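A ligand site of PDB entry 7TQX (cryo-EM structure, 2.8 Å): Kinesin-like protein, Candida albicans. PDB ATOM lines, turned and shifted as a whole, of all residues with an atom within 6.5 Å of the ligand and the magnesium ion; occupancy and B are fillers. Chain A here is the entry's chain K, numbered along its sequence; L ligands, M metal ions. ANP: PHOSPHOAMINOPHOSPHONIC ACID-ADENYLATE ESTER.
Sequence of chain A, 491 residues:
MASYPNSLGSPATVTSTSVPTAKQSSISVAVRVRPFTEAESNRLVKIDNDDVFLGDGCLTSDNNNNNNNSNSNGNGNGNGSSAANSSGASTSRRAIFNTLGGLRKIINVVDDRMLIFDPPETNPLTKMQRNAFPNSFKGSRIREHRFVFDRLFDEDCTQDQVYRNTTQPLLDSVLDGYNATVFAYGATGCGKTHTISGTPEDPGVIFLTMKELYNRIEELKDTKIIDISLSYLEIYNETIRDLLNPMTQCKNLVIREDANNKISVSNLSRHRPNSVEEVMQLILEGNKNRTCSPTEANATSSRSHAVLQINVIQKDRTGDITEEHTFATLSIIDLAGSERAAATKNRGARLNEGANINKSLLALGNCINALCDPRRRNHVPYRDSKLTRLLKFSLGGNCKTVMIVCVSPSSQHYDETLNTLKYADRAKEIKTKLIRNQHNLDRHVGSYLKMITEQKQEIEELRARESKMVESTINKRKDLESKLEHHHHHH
N of Gly 189 is in hydrogen-bond range of O2G of the ligand (3.4 Å). An oxygen (O1A) of the ligand lies within hydrogen-bond range of the backbone NH (N) of His 194, at 3.1 Å. An oxygen (O1B) of the ligand lies close to the side-chain hydroxyl of Thr 193 (3.0 Å).
The side-chain carboxylate of Glu 40 is in salt-bridge range of the guanidinium group of Arg 34. NH1 of Arg 32 lies close to NE2 of Gln 159, at 3.5 Å. The side-chain amide nitrogen (NE2) of Gln 159 is in hydrogen-bond range of the backbone carbonyl oxygen (O) of His 194 (2.9 Å). The side-chain hydroxyl (OG1) of Thr 195 is in hydrogen-bond range of the guanidinium group (NH1) of Arg 32. OG1 of Thr 195 sits at hydrogen-bond distance from O of Gly 191, 3.1 Å away. O of Gly 189 is in hydrogen-bond range of NE of Arg 34 (3.2 Å). The backbone NH (N) of Thr 37 lies within hydrogen-bond range of the side-chain carboxylate (OE1) of Glu 40 (2.7 Å).
The guanidinium group (NH2) of Arg 32 sits close to a nitrogen (N6) of the ligand (3.4 Å). Merely in contact with the ligand: Arg 34 (3.7 Å), Pro 35 (3.4 Å), Thr 37 (3.5 Å), Thr 188 (3.4 Å) and Gly 191 (3.4 Å). Within 4 Å of the ligand: Arg 32, Arg 34, Pro 35, Thr 37, Thr 188, Gly 189, Gly 191, Thr 193 and His 194.
Thr 193 touches the magnesium ion. Of the 25 residues printed, 1 comes within 4 Å of the magnesium ion. The nearest printed residue that does not touch the magnesium ion is Asn 298 (5.1 Å).
The magnesium ion is bound by an oxygen (O1G) of the ligand (2.0 Å), an oxygen (O1B) of the ligand (2.1 Å) and an oxygen (O2B) of the ligand (2.3 Å). The magnesium ion has three donor atoms within binding distance.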
ATOM      1  N   ARG A  32      20.695  -4.049  17.699  1.00  0.00           N
ATOM      2  CA  ARG A  32      21.121  -2.993  16.792  1.00  0.00           C
ATOM      3  C   ARG A  32      20.032  -1.926  16.688  1.00  0.00           C
ATOM      4  O   ARG A  32      18.867  -2.253  16.436  1.00  0.00           O
ATOM      5  CB  ARG A  32      21.442  -3.541  15.397  1.00  0.00           C
ATOM      6  CG  ARG A  32      22.231  -2.570  14.529  1.00  0.00           C
ATOM      7  CD  ARG A  32      22.347  -3.025  13.090  1.00  0.00           C
ATOM      8  NE  ARG A  32      23.318  -2.215  12.365  1.00  0.00           N
ATOM      9  CZ  ARG A  32      23.511  -2.250  11.055  1.00  0.00           C
ATOM     10  NH1 ARG A  32      22.793  -3.038  10.263  1.00  0.00           N
ATOM     11  NH2 ARG A  32      24.431  -1.459  10.509  1.00  0.00           N
ATOM     12  N   VAL A  33      20.433  -0.664  16.835  1.00  0.00           N
ATOM     13  CA  VAL A  33      19.531   0.474  16.742  1.00  0.00           C
ATOM     14  C   VAL A  33      19.652   1.061  15.342  1.00  0.00           C
ATOM     15  O   VAL A  33      20.743   1.427  14.906  1.00  0.00           O
ATOM     16  CB  VAL A  33      19.837   1.525  17.809  1.00  0.00           C
ATOM     17  CG1 VAL A  33      18.871   2.700  17.707  1.00  0.00           C
ATOM     18  CG2 VAL A  33      19.796   0.901  19.200  1.00  0.00           C
ATOM     19  N   ARG A  34      18.525   1.143  14.638  1.00  0.00           N
ATOM     20  CA  ARG A  34      18.520   1.688  13.284  1.00  0.00           C
ATOM     21  C   ARG A  34      18.814   3.199  13.322  1.00  0.00           C
ATOM     22  O   ARG A  34      18.440   3.882  14.276  1.00  0.00           O
ATOM     23  CB  ARG A  34      17.164   1.445  12.630  1.00  0.00           C
ATOM     24  CG  ARG A  34      17.011   1.985  11.227  1.00  0.00           C
ATOM     25  CD  ARG A  34      15.735   1.485  10.563  1.00  0.00           C
ATOM     26  NE  ARG A  34      14.540   2.084  11.147  1.00  0.00           N
ATOM     27  CZ  ARG A  34      14.134   3.336  10.938  1.00  0.00           C
ATOM     28  NH1 ARG A  34      14.818   4.164  10.157  1.00  0.00           N
ATOM     29  NH2 ARG A  34      13.023   3.757  11.511  1.00  0.00           N
ATOM     30  N   PRO A  35      19.495   3.742  12.304  1.00  0.00           N
ATOM     31  CA  PRO A  35      19.611   5.200  12.211  1.00  0.00           C
ATOM     32  C   PRO A  35      18.396   5.840  11.561  1.00  0.00           C
ATOM     33  O   PRO A  35      17.736   5.253  10.705  1.00  0.00           O
ATOM     34  CB  PRO A  35      20.862   5.400  11.353  1.00  0.00           C
ATOM     35  CG  PRO A  35      20.896   4.211  10.489  1.00  0.00           C
ATOM     36  CD  PRO A  35      20.388   3.079  11.334  1.00  0.00           C
ATOM     37  N   PHE A  36      18.115   7.071  11.993  1.00  0.00           N
ATOM     38  CA  PHE A  36      17.002   7.823  11.428  1.00  0.00           C
ATOM     39  C   PHE A  36      17.216   8.045   9.939  1.00  0.00           C
ATOM     40  O   PHE A  36      18.307   8.444   9.502  1.00  0.00           O
ATOM     41  CB  PHE A  36      16.846   9.171  12.127  1.00  0.00           C
ATOM     42  CG  PHE A  36      16.307   9.086  13.524  1.00  0.00           C
ATOM     43  CD1 PHE A  36      14.934   9.028  13.744  1.00  0.00           C
ATOM     44  CD2 PHE A  36      17.149   9.087  14.612  1.00  0.00           C
ATOM     45  CE1 PHE A  36      14.426   8.966  15.023  1.00  0.00           C
ATOM     46  CE2 PHE A  36      16.647   9.013  15.895  1.00  0.00           C
ATOM     47  CZ  PHE A  36      15.293   8.952  16.103  1.00  0.00           C
ATOM     48  N   THR A  37      16.167   7.806   9.145  1.00  0.00           N
ATOM     49  CA  THR A  37      16.216   8.140   7.739  1.00  0.00           C
ATOM     50  C   THR A  37      16.115   9.657   7.550  1.00  0.00           C
ATOM     51  O   THR A  37      15.685  10.389   8.445  1.00  0.00           O
ATOM     52  CB  THR A  37      15.083   7.443   6.976  1.00  0.00           C
ATOM     53  OG1 THR A  37      13.832   7.740   7.600  1.00  0.00           O
ATOM     54  CG2 THR A  37      15.303   5.946   6.959  1.00  0.00           C
ATOM     55  N   GLU A  40      12.788  10.845   7.898  1.00  0.00           N
ATOM     56  CA  GLU A  40      12.308  10.767   9.276  1.00  0.00           C
ATOM     57  C   GLU A  40      12.672  12.028  10.055  1.00  0.00           C
ATOM     58  O   GLU A  40      11.809  12.641  10.692  1.00  0.00           O
ATOM     59  CB  GLU A  40      12.898   9.541   9.987  1.00  0.00           C
ATOM     60  CG  GLU A  40      11.971   8.337  10.030  1.00  0.00           C
ATOM     61  CD  GLU A  40      12.667   7.074  10.511  1.00  0.00           C
ATOM     62  OE1 GLU A  40      13.893   6.948  10.328  1.00  0.00           O
ATOM     63  OE2 GLU A  40      11.972   6.203  11.081  1.00  0.00           O
ATOM     64  N   GLU A 155      23.745   4.161  16.844  1.00  0.00           N
ATOM     65  CA  GLU A 155      23.367   4.733  15.558  1.00  0.00           C
ATOM     66  C   GLU A 155      24.504   4.679  14.550  1.00  0.00           C
ATOM     67  O   GLU A 155      24.290   4.350  13.378  1.00  0.00           O
ATOM     68  CB  GLU A 155      22.898   6.178  15.749  1.00  0.00           C
ATOM     69  CG  GLU A 155      21.771   6.594  14.830  1.00  0.00           C
ATOM     70  CD  GLU A 155      21.245   7.982  15.131  1.00  0.00           C
ATOM     71  OE1 GLU A 155      21.788   8.635  16.040  1.00  0.00           O
ATOM     72  OE2 GLU A 155      20.300   8.417  14.450  1.00  0.00           O
ATOM     73  N   CYS A 157      27.046   2.687  14.295  1.00  0.00           N
ATOM     74  CA  CYS A 157      27.591   1.377  13.948  1.00  0.00           C
ATOM     75  C   CYS A 157      27.304   1.031  12.501  1.00  0.00           C
ATOM     76  O   CYS A 157      26.184   1.185  12.021  1.00  0.00           O
ATOM     77  CB  CYS A 157      27.008   0.304  14.880  1.00  0.00           C
ATOM     78  SG  CYS A 157      28.003  -0.018  16.348  1.00  0.00           S
ATOM     79  N   THR A 158      28.340   0.564  11.800  1.00  0.00           N
ATOM     80  CA  THR A 158      28.221   0.098  10.421  1.00  0.00           C
ATOM     81  C   THR A 158      28.095  -1.420  10.417  1.00  0.00           C
ATOM     82  O   THR A 158      27.973  -2.065  11.463  1.00  0.00           O
ATOM     83  CB  THR A 158      29.410   0.585   9.585  1.00  0.00           C
ATOM     84  OG1 THR A 158      29.196   0.231   8.213  1.00  0.00           O
ATOM     85  CG2 THR A 158      30.733  -0.018  10.042  1.00  0.00           C
ATOM     86  N   GLN A 159      28.098  -2.022   9.223  1.00  0.00           N
ATOM     87  CA  GLN A 159      27.833  -3.453   9.087  1.00  0.00           C
ATOM     88  C   GLN A 159      29.057  -4.310   9.325  1.00  0.00           C
ATOM     89  O   GLN A 159      28.920  -5.461   9.771  1.00  0.00           O
ATOM     90  CB  GLN A 159      27.282  -3.744   7.689  1.00  0.00           C
ATOM     91  CG  GLN A 159      26.107  -2.858   7.301  1.00  0.00           C
ATOM     92  CD  GLN A 159      25.071  -3.587   6.471  1.00  0.00           C
ATOM     93  OE1 GLN A 159      25.323  -3.939   5.311  1.00  0.00           O
ATOM     94  NE2 GLN A 159      23.906  -3.828   7.050  1.00  0.00           N
ATOM     95  N   GLY A 186      12.865  -8.702  14.672  1.00  0.00           N
ATOM     96  CA  GLY A 186      12.577  -7.280  14.656  1.00  0.00           C
ATOM     97  C   GLY A 186      11.185  -6.988  14.125  1.00  0.00           C
ATOM     98  O   GLY A 186      10.641  -7.763  13.321  1.00  0.00           O
ATOM     99  N   ALA A 187      10.597  -5.874  14.552  1.00  0.00           N
ATOM    100  CA  ALA A 187       9.250  -5.508  14.152  1.00  0.00           C
ATOM    101  C   ALA A 187       9.285  -4.848  12.777  1.00  0.00           C
ATOM    102  O   ALA A 187      10.302  -4.848  12.083  1.00  0.00           O
ATOM    103  CB  ALA A 187       8.619  -4.604  15.206  1.00  0.00           C
ATOM    104  N   THR A 188       8.157  -4.274  12.366  1.00  0.00           N
ATOM    105  CA  THR A 188       8.096  -3.591  11.078  1.00  0.00           C
ATOM    106  C   THR A 188       8.880  -2.280  11.139  1.00  0.00           C
ATOM    107  O   THR A 188       8.882  -1.576  12.148  1.00  0.00           O
ATOM    108  CB  THR A 188       6.647  -3.306  10.697  1.00  0.00           C
ATOM    109  OG1 THR A 188       5.930  -4.550  10.583  1.00  0.00           O
ATOM    110  CG2 THR A 188       6.558  -2.558   9.374  1.00  0.00           C
ATOM    111  N   GLY A 189       9.554  -1.953  10.031  1.00  0.00           N
ATOM    112  CA  GLY A 189      10.318  -0.721   9.959  1.00  0.00           C
ATOM    113  C   GLY A 189      11.471  -0.671  10.931  1.00  0.00           C
ATOM    114  O   GLY A 189      11.775   0.412  11.458  1.00  0.00           O
ATOM    115  N   CYS A 190      12.110  -1.804  11.188  1.00  0.00           N
ATOM    116  CA  CYS A 190      13.192  -1.901  12.165  1.00  0.00           C
ATOM    117  C   CYS A 190      14.574  -2.004  11.552  1.00  0.00           C
ATOM    118  O   CYS A 190      15.566  -1.789  12.251  1.00  0.00           O
ATOM    119  CB  CYS A 190      12.962  -3.127  13.059  1.00  0.00           C
ATOM    120  SG  CYS A 190      13.820  -4.593  12.458  1.00  0.00           S
ATOM    121  N   GLY A 191      14.674  -2.327  10.262  1.00  0.00           N
ATOM    122  CA  GLY A 191      15.952  -2.485   9.606  1.00  0.00           C
ATOM    123  C   GLY A 191      16.511  -3.891   9.593  1.00  0.00           C
ATOM    124  O   GLY A 191      17.720  -4.049   9.373  1.00  0.00           O
ATOM    125  N   LYS A 192      15.685  -4.908   9.831  1.00  0.00           N
ATOM    126  CA  LYS A 192      16.166  -6.286   9.799  1.00  0.00           C
ATOM    127  C   LYS A 192      16.680  -6.659   8.409  1.00  0.00           C
ATOM    128  O   LYS A 192      17.728  -7.303   8.280  1.00  0.00           O
ATOM    129  CB  LYS A 192      15.057  -7.237  10.233  1.00  0.00           C
ATOM    130  CG  LYS A 192      15.411  -8.713  10.146  1.00  0.00           C
ATOM    131  CD  LYS A 192      14.359  -9.574  10.829  1.00  0.00           C
ATOM    132  CE  LYS A 192      13.053  -9.576  10.069  1.00  0.00           C
ATOM    133  NZ  LYS A 192      12.193 -10.737  10.424  1.00  0.00           N
ATOM    134  N   THR A 193      15.943  -6.256   7.370  1.00  0.00           N
ATOM    135  CA  THR A 193      16.358  -6.581   6.006  1.00  0.00           C
ATOM    136  C   THR A 193      17.676  -5.920   5.668  1.00  0.00           C
ATOM    137  O   THR A 193      18.508  -6.499   4.964  1.00  0.00           O
ATOM    138  CB  THR A 193      15.274  -6.140   5.023  1.00  0.00           C
ATOM    139  OG1 THR A 193      14.062  -6.854   5.271  1.00  0.00           O
ATOM    140  CG2 THR A 193      15.711  -6.396   3.585  1.00  0.00           C
ATOM    141  N   HIS A 194      17.904  -4.704   6.163  1.00  0.00           N
ATOM    142  CA  HIS A 194      19.192  -4.042   5.963  1.00  0.00           C
ATOM    143  C   HIS A 194      20.313  -4.831   6.618  1.00  0.00           C
ATOM    144  O   HIS A 194      21.392  -4.972   6.047  1.00  0.00           O
ATOM    145  CB  HIS A 194      19.136  -2.621   6.507  1.00  0.00           C
ATOM    146  CG  HIS A 194      20.366  -1.820   6.218  1.00  0.00           C
ATOM    147  ND1 HIS A 194      20.594  -1.197   5.007  1.00  0.00           N
ATOM    148  CD2 HIS A 194      21.460  -1.550   6.984  1.00  0.00           C
ATOM    149  CE1 HIS A 194      21.751  -0.573   5.050  1.00  0.00           C
ATOM    150  NE2 HIS A 194      22.301  -0.771   6.227  1.00  0.00           N
ATOM    151  N   THR A 195      20.068  -5.346   7.826  1.00  0.00           N
ATOM    152  CA  THR A 195      21.136  -6.015   8.563  1.00  0.00           C
ATOM    153  C   THR A 195      21.477  -7.371   7.959  1.00  0.00           C
ATOM    154  O   THR A 195      22.650  -7.695   7.778  1.00  0.00           O
ATOM    155  CB  THR A 195      20.733  -6.162  10.030  1.00  0.00           C
ATOM    156  OG1 THR A 195      20.467  -4.873  10.593  1.00  0.00           O
ATOM    157  CG2 THR A 195      21.842  -6.837  10.826  1.00  0.00           C
ATOM    158  N   THR A 199      22.274  -3.996   0.955  1.00  0.00           N
ATOM    159  CA  THR A 199      22.224  -3.507  -0.416  1.00  0.00           C
ATOM    160  C   THR A 199      23.452  -4.003  -1.176  1.00  0.00           C
ATOM    161  O   THR A 199      24.415  -4.481  -0.567  1.00  0.00           O
ATOM    162  CB  THR A 199      22.182  -1.982  -0.444  1.00  0.00           C
ATOM    163  OG1 THR A 199      23.392  -1.453   0.124  1.00  0.00           O
ATOM    164  CG2 THR A 199      20.990  -1.457   0.341  1.00  0.00           C
ATOM    165  N   ASN A 298       2.205  -3.107   6.746  1.00  0.00           N
ATOM    166  CA  ASN A 298       2.964  -3.115   5.503  1.00  0.00           C
ATOM    167  C   ASN A 298       2.375  -4.175   4.572  1.00  0.00           C
ATOM    168  O   ASN A 298       1.793  -5.160   5.016  1.00  0.00           O
ATOM    169  CB  ASN A 298       4.448  -3.405   5.754  1.00  0.00           C
ATOM    170  CG  ASN A 298       5.327  -2.992   4.581  1.00  0.00           C
ATOM    171  OD1 ASN A 298       4.875  -2.957   3.437  1.00  0.00           O
ATOM    172  ND2 ASN A 298       6.586  -2.696   4.864  1.00  0.00           N
ATOM    173  N   THR A 300       4.022  -6.123   2.639  1.00  0.00           N
ATOM    174  CA  THR A 300       4.962  -7.259   2.459  1.00  0.00           C
ATOM    175  C   THR A 300       5.697  -7.474   3.776  1.00  0.00           C
ATOM    176  O   THR A 300       6.934  -7.280   3.800  1.00  0.00           O
ATOM    177  CB  THR A 300       5.897  -7.027   1.265  1.00  0.00           C
ATOM    178  OG1 THR A 300       6.905  -8.030   1.292  1.00  0.00           O
ATOM    179  CG2 THR A 300       6.536  -5.648   1.289  1.00  0.00           C
ATOM    180  N   SER A 301       4.980  -7.857   4.843  1.00  0.00           N
ATOM    181  CA  SER A 301       5.621  -7.968   6.189  1.00  0.00           C
ATOM    182  C   SER A 301       5.998  -9.423   6.527  1.00  0.00           C
ATOM    183  O   SER A 301       6.556  -9.626   7.615  1.00  0.00           O
ATOM    184  CB  SER A 301       4.716  -7.379   7.250  1.00  0.00           C
ATOM    185  OG  SER A 301       5.340  -7.431   8.529  1.00  0.00           O
HETATM  186  PG  ANP L   1      10.486  -4.562   7.239  1.00  0.00           P
HETATM  187  O1G ANP L   1      10.314  -5.154   5.873  1.00  0.00           O
HETATM  188  O2G ANP L   1       9.115  -4.661   8.019  1.00  0.00           O
HETATM  189  O3G ANP L   1      11.597  -5.362   8.016  1.00  0.00           O
HETATM  190  PB  ANP L   1      12.333  -2.839   6.176  1.00  0.00           P
HETATM  191  O1B ANP L   1      12.854  -4.199   5.887  1.00  0.00           O
HETATM  192  O2B ANP L   1      12.001  -2.122   4.827  1.00  0.00           O
HETATM  193  N3B ANP L   1      10.937  -2.938   7.103  1.00  0.00           N
HETATM  194  PA  ANP L   1      14.657  -1.467   6.104  1.00  0.00           P
HETATM  195  O1A ANP L   1      15.794  -2.406   6.162  1.00  0.00           O
HETATM  196  O2A ANP L   1      14.136  -1.197   4.693  1.00  0.00           O
HETATM  197  O3A ANP L   1      13.419  -2.016   6.936  1.00  0.00           O
HETATM  198  O5' ANP L   1      15.078  -0.132   6.838  1.00  0.00           O
HETATM  199  C5' ANP L   1      14.229   1.033   6.832  1.00  0.00           C
HETATM  200  C4' ANP L   1      14.967   2.172   6.169  1.00  0.00           C
HETATM  201  O4' ANP L   1      16.120   2.524   6.976  1.00  0.00           O
HETATM  202  C3' ANP L   1      15.489   1.892   4.770  1.00  0.00           C
HETATM  203  O3' ANP L   1      15.408   3.045   3.946  1.00  0.00           O
HETATM  204  C2' ANP L   1      16.939   1.475   5.022  1.00  0.00           C
HETATM  205  O2' ANP L   1      17.787   1.734   3.912  1.00  0.00           O
HETATM  206  C1' ANP L   1      17.301   2.364   6.208  1.00  0.00           C
HETATM  207  N9  ANP L   1      18.339   1.811   7.073  1.00  0.00           N
HETATM  208  C8  ANP L   1      18.206   0.765   7.947  1.00  0.00           C
HETATM  209  N7  ANP L   1      19.300   0.473   8.613  1.00  0.00           N
HETATM  210  C5  ANP L   1      20.223   1.400   8.133  1.00  0.00           C
HETATM  211  C6  ANP L   1      21.575   1.627   8.437  1.00  0.00           C
HETATM  212  N6  ANP L   1      22.277   0.909   9.321  1.00  0.00           N
HETATM  213  N1  ANP L   1      22.204   2.634   7.781  1.00  0.00           N
HETATM  214  C2  ANP L   1      21.511   3.355   6.893  1.00  0.00           C
HETATM  215  N3  ANP L   1      20.234   3.232   6.532  1.00  0.00           N
HETATM  216  C4  ANP L   1      19.641   2.229   7.193  1.00  0.00           C
HETATM  217 MG    MG M   1      11.415  -4.340   4.366  1.00  0.00          MG
